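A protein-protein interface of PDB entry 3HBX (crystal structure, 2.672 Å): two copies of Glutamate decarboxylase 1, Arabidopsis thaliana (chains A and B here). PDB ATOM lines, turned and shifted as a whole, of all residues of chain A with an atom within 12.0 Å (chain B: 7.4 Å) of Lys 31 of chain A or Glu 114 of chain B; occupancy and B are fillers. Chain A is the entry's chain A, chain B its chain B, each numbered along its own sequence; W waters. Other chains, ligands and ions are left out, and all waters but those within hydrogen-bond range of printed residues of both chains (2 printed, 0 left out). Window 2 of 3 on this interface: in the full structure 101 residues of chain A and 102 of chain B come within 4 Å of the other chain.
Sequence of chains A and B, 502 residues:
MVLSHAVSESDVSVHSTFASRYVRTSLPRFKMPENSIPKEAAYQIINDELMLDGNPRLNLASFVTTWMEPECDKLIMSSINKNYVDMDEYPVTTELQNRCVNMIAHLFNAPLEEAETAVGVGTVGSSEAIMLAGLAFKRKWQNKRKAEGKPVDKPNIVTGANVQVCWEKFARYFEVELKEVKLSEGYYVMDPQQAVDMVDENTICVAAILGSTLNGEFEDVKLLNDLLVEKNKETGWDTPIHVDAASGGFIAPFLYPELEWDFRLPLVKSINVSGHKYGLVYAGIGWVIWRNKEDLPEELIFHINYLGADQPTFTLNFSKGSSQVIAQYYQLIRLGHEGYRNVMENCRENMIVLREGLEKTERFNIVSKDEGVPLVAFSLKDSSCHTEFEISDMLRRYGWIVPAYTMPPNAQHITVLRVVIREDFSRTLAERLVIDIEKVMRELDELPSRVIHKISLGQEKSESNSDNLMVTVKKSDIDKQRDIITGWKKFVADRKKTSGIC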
ATOM      1  N   THR A  25     -20.191  21.864  -5.364  1.00  0.00           N
ATOM      2  CA  THR A  25     -18.770  21.920  -5.052  1.00  0.00           C
ATOM      3  C   THR A  25     -18.284  20.547  -4.618  1.00  0.00           C
ATOM      4  O   THR A  25     -18.953  19.857  -3.848  1.00  0.00           O
ATOM      5  CB  THR A  25     -18.479  22.925  -3.925  1.00  0.00           C
ATOM      6  OG1 THR A  25     -19.188  24.147  -4.170  1.00  0.00           O
ATOM      7  CG2 THR A  25     -16.982  23.210  -3.836  1.00  0.00           C
ATOM      8  N   SER A  26     -17.122  20.144  -5.122  1.00  0.00           N
ATOM      9  CA  SER A  26     -16.510  18.897  -4.689  1.00  0.00           C
ATOM     10  C   SER A  26     -15.848  19.094  -3.331  1.00  0.00           C
ATOM     11  O   SER A  26     -15.413  20.198  -2.999  1.00  0.00           O
ATOM     12  CB  SER A  26     -15.498  18.401  -5.724  1.00  0.00           C
ATOM     13  OG  SER A  26     -14.752  19.477  -6.263  1.00  0.00           O
ATOM     14  N   LEU A  27     -15.783  18.022  -2.548  1.00  0.00           N
ATOM     15  CA  LEU A  27     -15.216  18.085  -1.203  1.00  0.00           C
ATOM     16  C   LEU A  27     -13.744  18.501  -1.208  1.00  0.00           C
ATOM     17  O   LEU A  27     -12.963  18.030  -2.038  1.00  0.00           O
ATOM     18  CB  LEU A  27     -15.382  16.736  -0.501  1.00  0.00           C
ATOM     19  CG  LEU A  27     -16.823  16.312  -0.211  1.00  0.00           C
ATOM     20  CD1 LEU A  27     -16.935  14.796  -0.067  1.00  0.00           C
ATOM     21  CD2 LEU A  27     -17.361  17.028   1.026  1.00  0.00           C
ATOM     22  N   PRO A  28     -13.365  19.388  -0.274  1.00  0.00           N
ATOM     23  CA  PRO A  28     -11.996  19.899  -0.142  1.00  0.00           C
ATOM     24  C   PRO A  28     -10.974  18.775   0.001  1.00  0.00           C
ATOM     25  O   PRO A  28     -11.215  17.814   0.732  1.00  0.00           O
ATOM     26  CB  PRO A  28     -12.054  20.726   1.144  1.00  0.00           C
ATOM     27  CG  PRO A  28     -13.479  21.126   1.270  1.00  0.00           C
ATOM     28  CD  PRO A  28     -14.272  19.973   0.729  1.00  0.00           C
ATOM     29  N   ARG A  29      -9.848  18.899  -0.696  1.00  0.00           N
ATOM     30  CA  ARG A  29      -8.802  17.883  -0.654  1.00  0.00           C
ATOM     31  C   ARG A  29      -7.555  18.368   0.079  1.00  0.00           C
ATOM     32  O   ARG A  29      -6.802  17.565   0.625  1.00  0.00           O
ATOM     33  CB  ARG A  29      -8.411  17.448  -2.070  1.00  0.00           C
ATOM     34  CG  ARG A  29      -9.386  16.497  -2.741  1.00  0.00           C
ATOM     35  CD  ARG A  29      -8.906  16.133  -4.142  1.00  0.00           C
ATOM     36  NE  ARG A  29      -9.846  15.263  -4.847  1.00  0.00           N
ATOM     37  CZ  ARG A  29      -9.709  13.944  -4.955  1.00  0.00           C
ATOM     38  NH1 ARG A  29      -8.667  13.336  -4.401  1.00  0.00           N
ATOM     39  NH2 ARG A  29     -10.613  13.232  -5.617  1.00  0.00           N
ATOM     40  N   PHE A  30      -7.339  19.679   0.088  1.00  0.00           N
ATOM     41  CA  PHE A  30      -6.082  20.229   0.582  1.00  0.00           C
ATOM     42  C   PHE A  30      -6.250  21.218   1.732  1.00  0.00           C
ATOM     43  O   PHE A  30      -5.626  21.063   2.781  1.00  0.00           O
ATOM     44  CB  PHE A  30      -5.302  20.878  -0.562  1.00  0.00           C
ATOM     45  CG  PHE A  30      -5.027  19.950  -1.708  1.00  0.00           C
ATOM     46  CD1 PHE A  30      -3.974  19.049  -1.650  1.00  0.00           C
ATOM     47  CD2 PHE A  30      -5.821  19.973  -2.844  1.00  0.00           C
ATOM     48  CE1 PHE A  30      -3.719  18.187  -2.706  1.00  0.00           C
ATOM     49  CE2 PHE A  30      -5.569  19.116  -3.904  1.00  0.00           C
ATOM     50  CZ  PHE A  30      -4.517  18.221  -3.834  1.00  0.00           C
ATOM     51  N   LYS A  31      -7.082  22.235   1.533  1.00  0.00           N
ATOM     52  CA  LYS A  31      -7.281  23.262   2.553  1.00  0.00           C
ATOM     53  C   LYS A  31      -8.592  23.092   3.306  1.00  0.00           C
ATOM     54  O   LYS A  31      -9.606  22.694   2.735  1.00  0.00           O
ATOM     55  CB  LYS A  31      -7.231  24.662   1.935  1.00  0.00           C
ATOM     56  CG  LYS A  31      -5.838  25.167   1.611  1.00  0.00           C
ATOM     57  CD  LYS A  31      -5.883  26.627   1.185  1.00  0.00           C
ATOM     58  CE  LYS A  31      -4.497  27.162   0.858  1.00  0.00           C
ATOM     59  NZ  LYS A  31      -4.542  28.596   0.452  1.00  0.00           N
ATOM     60  N   MET A  32      -8.564  23.406   4.594  1.00  0.00           N
ATOM     61  CA  MET A  32      -9.773  23.421   5.403  1.00  0.00           C
ATOM     62  C   MET A  32     -10.643  24.606   4.988  1.00  0.00           C
ATOM     63  O   MET A  32     -10.145  25.723   4.836  1.00  0.00           O
ATOM     64  CB  MET A  32      -9.408  23.516   6.888  1.00  0.00           C
ATOM     65  CG  MET A  32     -10.586  23.381   7.836  1.00  0.00           C
ATOM     66  SD  MET A  32     -10.074  23.365   9.564  1.00  0.00           S
ATOM     67  CE  MET A  32      -9.219  24.929   9.671  1.00  0.00           C
ATOM     68  N   PRO A  33     -11.947  24.362   4.788  1.00  0.00           N
ATOM     69  CA  PRO A  33     -12.888  25.408   4.373  1.00  0.00           C
ATOM     70  C   PRO A  33     -12.956  26.540   5.392  1.00  0.00           C
ATOM     71  O   PRO A  33     -12.777  26.301   6.585  1.00  0.00           O
ATOM     72  CB  PRO A  33     -14.232  24.672   4.324  1.00  0.00           C
ATOM     73  CG  PRO A  33     -13.881  23.235   4.174  1.00  0.00           C
ATOM     74  CD  PRO A  33     -12.608  23.055   4.936  1.00  0.00           C
ATOM     75  N   GLU A  34     -13.212  27.756   4.924  1.00  0.00           N
ATOM     76  CA  GLU A  34     -13.323  28.904   5.815  1.00  0.00           C
ATOM     77  C   GLU A  34     -14.648  28.904   6.567  1.00  0.00           C
ATOM     78  O   GLU A  34     -14.698  29.244   7.749  1.00  0.00           O
ATOM     79  CB  GLU A  34     -13.165  30.210   5.031  1.00  0.00           C
ATOM     80  CG  GLU A  34     -11.724  30.569   4.697  1.00  0.00           C
ATOM     81  CD  GLU A  34     -10.947  31.069   5.905  1.00  0.00           C
ATOM     82  OE1 GLU A  34     -11.586  31.458   6.907  1.00  0.00           O
ATOM     83  OE2 GLU A  34      -9.698  31.078   5.848  1.00  0.00           O
ATOM     84  N   ASN A  35     -15.716  28.513   5.881  1.00  0.00           N
ATOM     85  CA  ASN A  35     -17.059  28.584   6.449  1.00  0.00           C
ATOM     86  C   ASN A  35     -17.707  27.225   6.695  1.00  0.00           C
ATOM     87  O   ASN A  35     -17.370  26.234   6.047  1.00  0.00           O
ATOM     88  CB  ASN A  35     -17.967  29.432   5.555  1.00  0.00           C
ATOM     89  CG  ASN A  35     -17.575  30.897   5.550  1.00  0.00           C
ATOM     90  OD1 ASN A  35     -17.380  31.494   4.490  1.00  0.00           O
ATOM     91  ND2 ASN A  35     -17.449  31.483   6.737  1.00  0.00           N
ATOM     92  N   SER A  36     -18.644  27.194   7.636  1.00  0.00           N
ATOM     93  CA  SER A  36     -19.395  25.983   7.935  1.00  0.00           C
ATOM     94  C   SER A  36     -20.403  25.685   6.834  1.00  0.00           C
ATOM     95  O   SER A  36     -20.801  26.576   6.084  1.00  0.00           O
ATOM     96  CB  SER A  36     -20.131  26.129   9.265  1.00  0.00           C
ATOM     97  OG  SER A  36     -19.239  26.447  10.318  1.00  0.00           O
ATOM     98  N   ILE A  37     -20.805  24.423   6.738  1.00  0.00           N
ATOM     99  CA  ILE A  37     -21.902  24.032   5.864  1.00  0.00           C
ATOM    100  C   ILE A  37     -22.892  23.205   6.678  1.00  0.00           C
ATOM    101  O   ILE A  37     -22.518  22.604   7.682  1.00  0.00           O
ATOM    102  CB  ILE A  37     -21.416  23.241   4.625  1.00  0.00           C
ATOM    103  CG1 ILE A  37     -21.002  21.818   5.008  1.00  0.00           C
ATOM    104  CG2 ILE A  37     -20.274  23.973   3.931  1.00  0.00           C
ATOM    105  CD1 ILE A  37     -20.544  20.981   3.820  1.00  0.00           C
ATOM    106  N   ILE A  46     -20.315  13.277   2.092  1.00  0.00           N
ATOM    107  CA  ILE A  46     -19.319  12.340   2.600  1.00  0.00           C
ATOM    108  C   ILE A  46     -19.841  10.911   2.515  1.00  0.00           C
ATOM    109  O   ILE A  46     -19.121   9.996   2.112  1.00  0.00           O
ATOM    110  CB  ILE A  46     -18.921  12.659   4.052  1.00  0.00           C
ATOM    111  CG1 ILE A  46     -18.107  13.951   4.105  1.00  0.00           C
ATOM    112  CG2 ILE A  46     -18.120  11.516   4.651  1.00  0.00           C
ATOM    113  CD1 ILE A  46     -17.778  14.397   5.510  1.00  0.00           C
ATOM    114  N   ARG B  99      -6.541  13.663   3.018  1.00  0.00           N
ATOM    115  CA  ARG B  99      -7.076  15.019   3.012  1.00  0.00           C
ATOM    116  C   ARG B  99      -6.951  15.666   4.387  1.00  0.00           C
ATOM    117  O   ARG B  99      -6.630  16.848   4.496  1.00  0.00           O
ATOM    118  CB  ARG B  99      -8.535  15.024   2.551  1.00  0.00           C
ATOM    119  CG  ARG B  99      -8.725  14.512   1.136  1.00  0.00           C
ATOM    120  CD  ARG B  99     -10.189  14.465   0.747  1.00  0.00           C
ATOM    121  NE  ARG B  99     -10.393  13.666  -0.457  1.00  0.00           N
ATOM    122  CZ  ARG B  99     -11.584  13.380  -0.973  1.00  0.00           C
ATOM    123  NH1 ARG B  99     -12.685  13.833  -0.392  1.00  0.00           N
ATOM    124  NH2 ARG B  99     -11.674  12.644  -2.070  1.00  0.00           N
ATOM    125  N   ASN B 102      -3.402  16.718   4.843  1.00  0.00           N
ATOM    126  CA  ASN B 102      -3.196  17.945   4.086  1.00  0.00           C
ATOM    127  C   ASN B 102      -3.762  19.158   4.814  1.00  0.00           C
ATOM    128  O   ASN B 102      -3.083  20.168   4.983  1.00  0.00           O
ATOM    129  CB  ASN B 102      -3.832  17.836   2.698  1.00  0.00           C
ATOM    130  CG  ASN B 102      -3.130  16.828   1.810  1.00  0.00           C
ATOM    131  OD1 ASN B 102      -2.041  16.353   2.130  1.00  0.00           O
ATOM    132  ND2 ASN B 102      -3.753  16.497   0.684  1.00  0.00           N
ATOM    133  N   MET B 103      -5.011  19.045   5.249  1.00  0.00           N
ATOM    134  CA  MET B 103      -5.703  20.166   5.870  1.00  0.00           C
ATOM    135  C   MET B 103      -5.058  20.571   7.186  1.00  0.00           C
ATOM    136  O   MET B 103      -4.942  21.756   7.487  1.00  0.00           O
ATOM    137  CB  MET B 103      -7.187  19.843   6.062  1.00  0.00           C
ATOM    138  CG  MET B 103      -7.943  19.689   4.752  1.00  0.00           C
ATOM    139  SD  MET B 103      -9.733  19.642   4.936  1.00  0.00           S
ATOM    140  CE  MET B 103      -9.972  17.988   5.573  1.00  0.00           C
ATOM    141  N   ILE B 104      -4.635  19.584   7.968  1.00  0.00           N
ATOM    142  CA  ILE B 104      -3.960  19.857   9.230  1.00  0.00           C
ATOM    143  C   ILE B 104      -2.574  20.435   8.971  1.00  0.00           C
ATOM    144  O   ILE B 104      -2.115  21.324   9.689  1.00  0.00           O
ATOM    145  CB  ILE B 104      -3.861  18.593  10.111  1.00  0.00           C
ATOM    146  CG1 ILE B 104      -5.259  18.152  10.554  1.00  0.00           C
ATOM    147  CG2 ILE B 104      -2.993  18.854  11.328  1.00  0.00           C
ATOM    148  CD1 ILE B 104      -5.287  16.830  11.287  1.00  0.00           C
ATOM    149  N   HIS B 106      -1.588  22.308   6.384  1.00  0.00           N
ATOM    150  CA  HIS B 106      -1.778  23.712   6.034  1.00  0.00           C
ATOM    151  C   HIS B 106      -2.177  24.524   7.260  1.00  0.00           C
ATOM    152  O   HIS B 106      -1.757  25.669   7.423  1.00  0.00           O
ATOM    153  CB  HIS B 106      -2.838  23.865   4.940  1.00  0.00           C
ATOM    154  CG  HIS B 106      -2.316  23.632   3.554  1.00  0.00           C
ATOM    155  ND1 HIS B 106      -2.458  22.430   2.895  1.00  0.00           N
ATOM    156  CD2 HIS B 106      -1.654  24.451   2.702  1.00  0.00           C
ATOM    157  CE1 HIS B 106      -1.905  22.517   1.698  1.00  0.00           C
ATOM    158  NE2 HIS B 106      -1.411  23.734   1.556  1.00  0.00           N
ATOM    159  N   LEU B 107      -2.988  23.921   8.121  1.00  0.00           N
ATOM    160  CA  LEU B 107      -3.430  24.580   9.338  1.00  0.00           C
ATOM    161  C   LEU B 107      -2.232  24.953  10.201  1.00  0.00           C
ATOM    162  O   LEU B 107      -2.253  25.959  10.915  1.00  0.00           O
ATOM    163  CB  LEU B 107      -4.384  23.673  10.117  1.00  0.00           C
ATOM    164  CG  LEU B 107      -5.094  24.309  11.314  1.00  0.00           C
ATOM    165  CD1 LEU B 107      -5.968  25.467  10.859  1.00  0.00           C
ATOM    166  CD2 LEU B 107      -5.917  23.273  12.067  1.00  0.00           C
ATOM    167  N   LEU B 112       4.112  24.014   2.109  1.00  0.00           N
ATOM    168  CA  LEU B 112       3.469  23.240   1.051  1.00  0.00           C
ATOM    169  C   LEU B 112       3.088  24.106  -0.141  1.00  0.00           C
ATOM    170  O   LEU B 112       2.482  25.166   0.018  1.00  0.00           O
ATOM    171  CB  LEU B 112       2.221  22.535   1.585  1.00  0.00           C
ATOM    172  CG  LEU B 112       2.434  21.349   2.525  1.00  0.00           C
ATOM    173  CD1 LEU B 112       1.098  20.874   3.070  1.00  0.00           C
ATOM    174  CD2 LEU B 112       3.166  20.220   1.812  1.00  0.00           C
ATOM    175  N   GLU B 113       3.444  23.645  -1.334  1.00  0.00           N
ATOM    176  CA  GLU B 113       3.030  24.315  -2.557  1.00  0.00           C
ATOM    177  C   GLU B 113       1.571  23.969  -2.830  1.00  0.00           C
ATOM    178  O   GLU B 113       1.062  22.969  -2.322  1.00  0.00           O
ATOM    179  CB  GLU B 113       3.916  23.894  -3.732  1.00  0.00           C
ATOM    180  CG  GLU B 113       3.645  24.653  -5.024  1.00  0.00           C
ATOM    181  CD  GLU B 113       4.603  24.278  -6.139  1.00  0.00           C
ATOM    182  OE1 GLU B 113       5.729  23.827  -5.834  1.00  0.00           O
ATOM    183  OE2 GLU B 113       4.231  24.436  -7.323  1.00  0.00           O
ATOM    184  N   GLU B 114       0.896  24.799  -3.617  1.00  0.00           N
ATOM    185  CA  GLU B 114      -0.505  24.561  -3.944  1.00  0.00           C
ATOM    186  C   GLU B 114      -0.718  23.169  -4.529  1.00  0.00           C
ATOM    187  O   GLU B 114      -0.072  22.789  -5.508  1.00  0.00           O
ATOM    188  CB  GLU B 114      -1.023  25.631  -4.909  1.00  0.00           C
ATOM    189  CG  GLU B 114      -1.471  26.910  -4.222  1.00  0.00           C
ATOM    190  CD  GLU B 114      -2.712  26.707  -3.375  1.00  0.00           C
ATOM    191  OE1 GLU B 114      -3.558  25.869  -3.754  1.00  0.00           O
ATOM    192  OE2 GLU B 114      -2.844  27.386  -2.333  1.00  0.00           O
ATOM    193  N   ALA B 115      -1.623  22.414  -3.910  1.00  0.00           N
ATOM    194  CA  ALA B 115      -1.983  21.070  -4.365  1.00  0.00           C
ATOM    195  C   ALA B 115      -0.888  20.029  -4.125  1.00  0.00           C
ATOM    196  O   ALA B 115      -0.922  18.940  -4.699  1.00  0.00           O
ATOM    197  CB  ALA B 115      -2.400  21.089  -5.834  1.00  0.00           C
ATOM    198  N   GLU B 116       0.077  20.363  -3.275  1.00  0.00           N
ATOM    199  CA  GLU B 116       1.128  19.422  -2.903  1.00  0.00           C
ATOM    200  C   GLU B 116       0.639  18.508  -1.783  1.00  0.00           C
ATOM    201  O   GLU B 116      -0.105  18.942  -0.904  1.00  0.00           O
ATOM    202  CB  GLU B 116       2.391  20.170  -2.465  1.00  0.00           C
ATOM    203  CG  GLU B 116       3.559  19.273  -2.075  1.00  0.00           C
ATOM    204  CD  GLU B 116       4.846  20.052  -1.850  1.00  0.00           C
ATOM    205  OE1 GLU B 116       4.891  21.247  -2.216  1.00  0.00           O
ATOM    206  OE2 GLU B 116       5.813  19.470  -1.311  1.00  0.00           O
ATOM    207  N   THR B 117       1.049  17.244  -1.820  1.00  0.00           N
ATOM    208  CA  THR B 117       0.656  16.291  -0.786  1.00  0.00           C
ATOM    209  C   THR B 117       1.531  16.430   0.457  1.00  0.00           C
ATOM    210  O   THR B 117       2.760  16.361   0.379  1.00  0.00           O
ATOM    211  CB  THR B 117       0.707  14.839  -1.293  1.00  0.00           C
ATOM    212  OG1 THR B 117      -0.241  14.671  -2.354  1.00  0.00           O
ATOM    213  CG2 THR B 117       0.371  13.871  -0.168  1.00  0.00           C
ATOM    214  N   LEU B 332     -14.038  18.590   9.974  1.00  0.00           N
ATOM    215  CA  LEU B 332     -13.234  19.570   9.254  1.00  0.00           C
ATOM    216  C   LEU B 332     -14.029  20.324   8.182  1.00  0.00           C
ATOM    217  O   LEU B 332     -14.061  21.552   8.182  1.00  0.00           O
ATOM    218  CB  LEU B 332     -11.988  18.912   8.655  1.00  0.00           C
ATOM    219  CG  LEU B 332     -10.931  18.441   9.662  1.00  0.00           C
ATOM    220  CD1 LEU B 332      -9.758  17.782   8.953  1.00  0.00           C
ATOM    221  CD2 LEU B 332     -10.445  19.596  10.517  1.00  0.00           C
ATOM    222  N   ILE B 333     -14.677  19.595   7.280  1.00  0.00           N
ATOM    223  CA  ILE B 333     -15.396  20.232   6.179  1.00  0.00           C
ATOM    224  C   ILE B 333     -16.769  20.767   6.585  1.00  0.00           C
ATOM    225  O   ILE B 333     -17.318  21.650   5.925  1.00  0.00           O
ATOM    226  CB  ILE B 333     -15.527  19.297   4.955  1.00  0.00           C
ATOM    227  CG1 ILE B 333     -16.370  18.068   5.292  1.00  0.00           C
ATOM    228  CG2 ILE B 333     -14.154  18.885   4.448  1.00  0.00           C
ATOM    229  CD1 ILE B 333     -17.844  18.230   4.994  1.00  0.00           C
ATOM    230  N   HIS B 337     -13.074  26.735   9.413  1.00  0.00           N
ATOM    231  CA  HIS B 337     -12.479  27.684  10.348  1.00  0.00           C
ATOM    232  C   HIS B 337     -13.554  28.310  11.230  1.00  0.00           C
ATOM    233  O   HIS B 337     -13.392  28.419  12.447  1.00  0.00           O
ATOM    234  CB  HIS B 337     -11.729  28.788   9.600  1.00  0.00           C
ATOM    235  CG  HIS B 337     -10.352  28.397   9.154  1.00  0.00           C
ATOM    236  ND1 HIS B 337      -9.242  28.541   9.957  1.00  0.00           N
ATOM    237  CD2 HIS B 337      -9.907  27.880   7.985  1.00  0.00           C
ATOM    238  CE1 HIS B 337      -8.172  28.123   9.305  1.00  0.00           C
ATOM    239  NE2 HIS B 337      -8.548  27.717   8.104  1.00  0.00           N
HETATM  240  O   HOH W   1      -6.383  24.130   6.297  1.00  0.00           O
HETATM  241  O   HOH W   2      -7.709  12.595  -1.726  1.00  0.00           O
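The side-chain amide nitrogen of Asn 102 of chain B is in hydrogen-bond range of the backbone carbonyl oxygen of Arg 29 of chain A (3.2 Å). The backbone NH (N) of Met 103 of chain B sits close to the backbone carbonyl oxygen (O) of Phe 30 of chain A (3.2 Å). The backbone carbonyl oxygen (O) of Phe 30 of chain A is in hydrogen-bond range of a ring nitrogen (ND1) of His 106 of chain B, 3.5 Å away. NZ of Lys 31 of chain A lies within salt-bridge range of OE2 of Glu 114 of chain B. The backbone carbonyl oxygen of Pro 33 of chain A sits at hydrogen-bond distance from the backbone NH of His 337 of chain B, 2.9 Å away. O of Glu 34 of chain A is in hydrogen-bond range of N of His 337 of chain B. The backbone carbonyl oxygen (O) of Asn 102 of chain B sits close to the backbone carbonyl oxygen (O) of Phe 30 of chain A. The backbone carbonyl oxygen of Lys 31 of chain A sits close to the side-chain sulfur of Met 103 of chain B (3.8 Å).
The backbone carbonyl oxygen of Asn 102 of chain B sits at hydrogen-bond distance from a ring nitrogen (ND1) of His 106 of chain B (3.1 Å). OE1 of Glu 116 of chain B sits at hydrogen-bond distance from N of Glu 113 of chain B (2.9 Å).
Among the printed residues, pairs that only touch across the chains: Met 32 of chain A with His 337 of chain B, Arg 29 of chain A with Arg 99 of chain B, Pro 28 of chain A with Arg 99 of chain B, Met 32 of chain A with Leu 107 of chain B, Phe 30 of chain A with Ala 115 of chain B, Met 32 of chain A with Met 103 of chain B, Ile 37 of chain A with Ile 333 of chain B, Pro 33 of chain A with Leu 332 of chain B, Ile 46 of chain A with Ile 333 of chain B, Pro 28 of chain A with Ile 333 of chain B, Met 32 of chain A with Leu 332 of chain B, Pro 33 of chain A with Ile 333 of chain B, Phe 30 of chain A with Glu 116 of chain B and Leu 27 of chain A with Arg 99 of chain B.
Lys 31 of chain A touches just these residues of chain B: Met 103 (3.8 Å) and Glu 114 (3.5 Å). Of chain A, only Lys 31 comes within 4 Å of Glu 114 of chain B. Met 103 of chain B touches three residues of chain A. Of chain A, only Phe 30 (3.5 Å) comes within 4 Å of His 106 of chain B. No residue of chain A comes within 4 Å of Leu 112 of chain B. No residue of chain A comes within 4 Å of Glu 113 of chain B. Of chain A, only Phe 30 comes within 4 Å of Ala 115 of chain B. Of the printed residues of chain B, Leu 27 of chain A touches Arg 99 (3.96 Å). Printed residues of chain A within 4 Å of Leu 107 of chain B: Met 32 (3.5 Å). Of the printed residues of chain B, Phe 30 of chain A touches Asn 102 (3.4 Å), Met 103 (3.2 Å), His 106 (3.5 Å), Ala 115 (3.5 Å) and Glu 116 (3.9 Å). Thr 25 of chain A touches none of the printed residues of chain B.
Hydrophobic or aromatic side chains of chain A that line the printed part of chain B: Leu 27, Pro 28, Phe 30, Met 32, Pro 33, Ile 37 and Ile 46. Among the printed residues, 22 pairs touch across the chains. Among the printed residues, Asp or Glu carboxylates within 4 Å of a Lys or Arg side-chain nitrogen of the other chain: Lys 31 of chain A with Glu 114 of chain B (3.5 Å).
No position is printed for both chains. Of the 22 pairs that touch across the chains among the printed residues, none has its exchanged pair printed and touching as well.
Water W1 lies within hydrogen-bond range of the backbone NH (N) of Met 32 of chain A (2.9 Å) and the backbone carbonyl oxygen (O) of Met 103 of chain B (3.0 Å). Water W2 lies within hydrogen-bond range of the guanidinium group (NH1) of Arg 29 of chain A (2.9 Å) and the guanidinium group (NE) of Arg 99 of chain B (3.2 Å).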
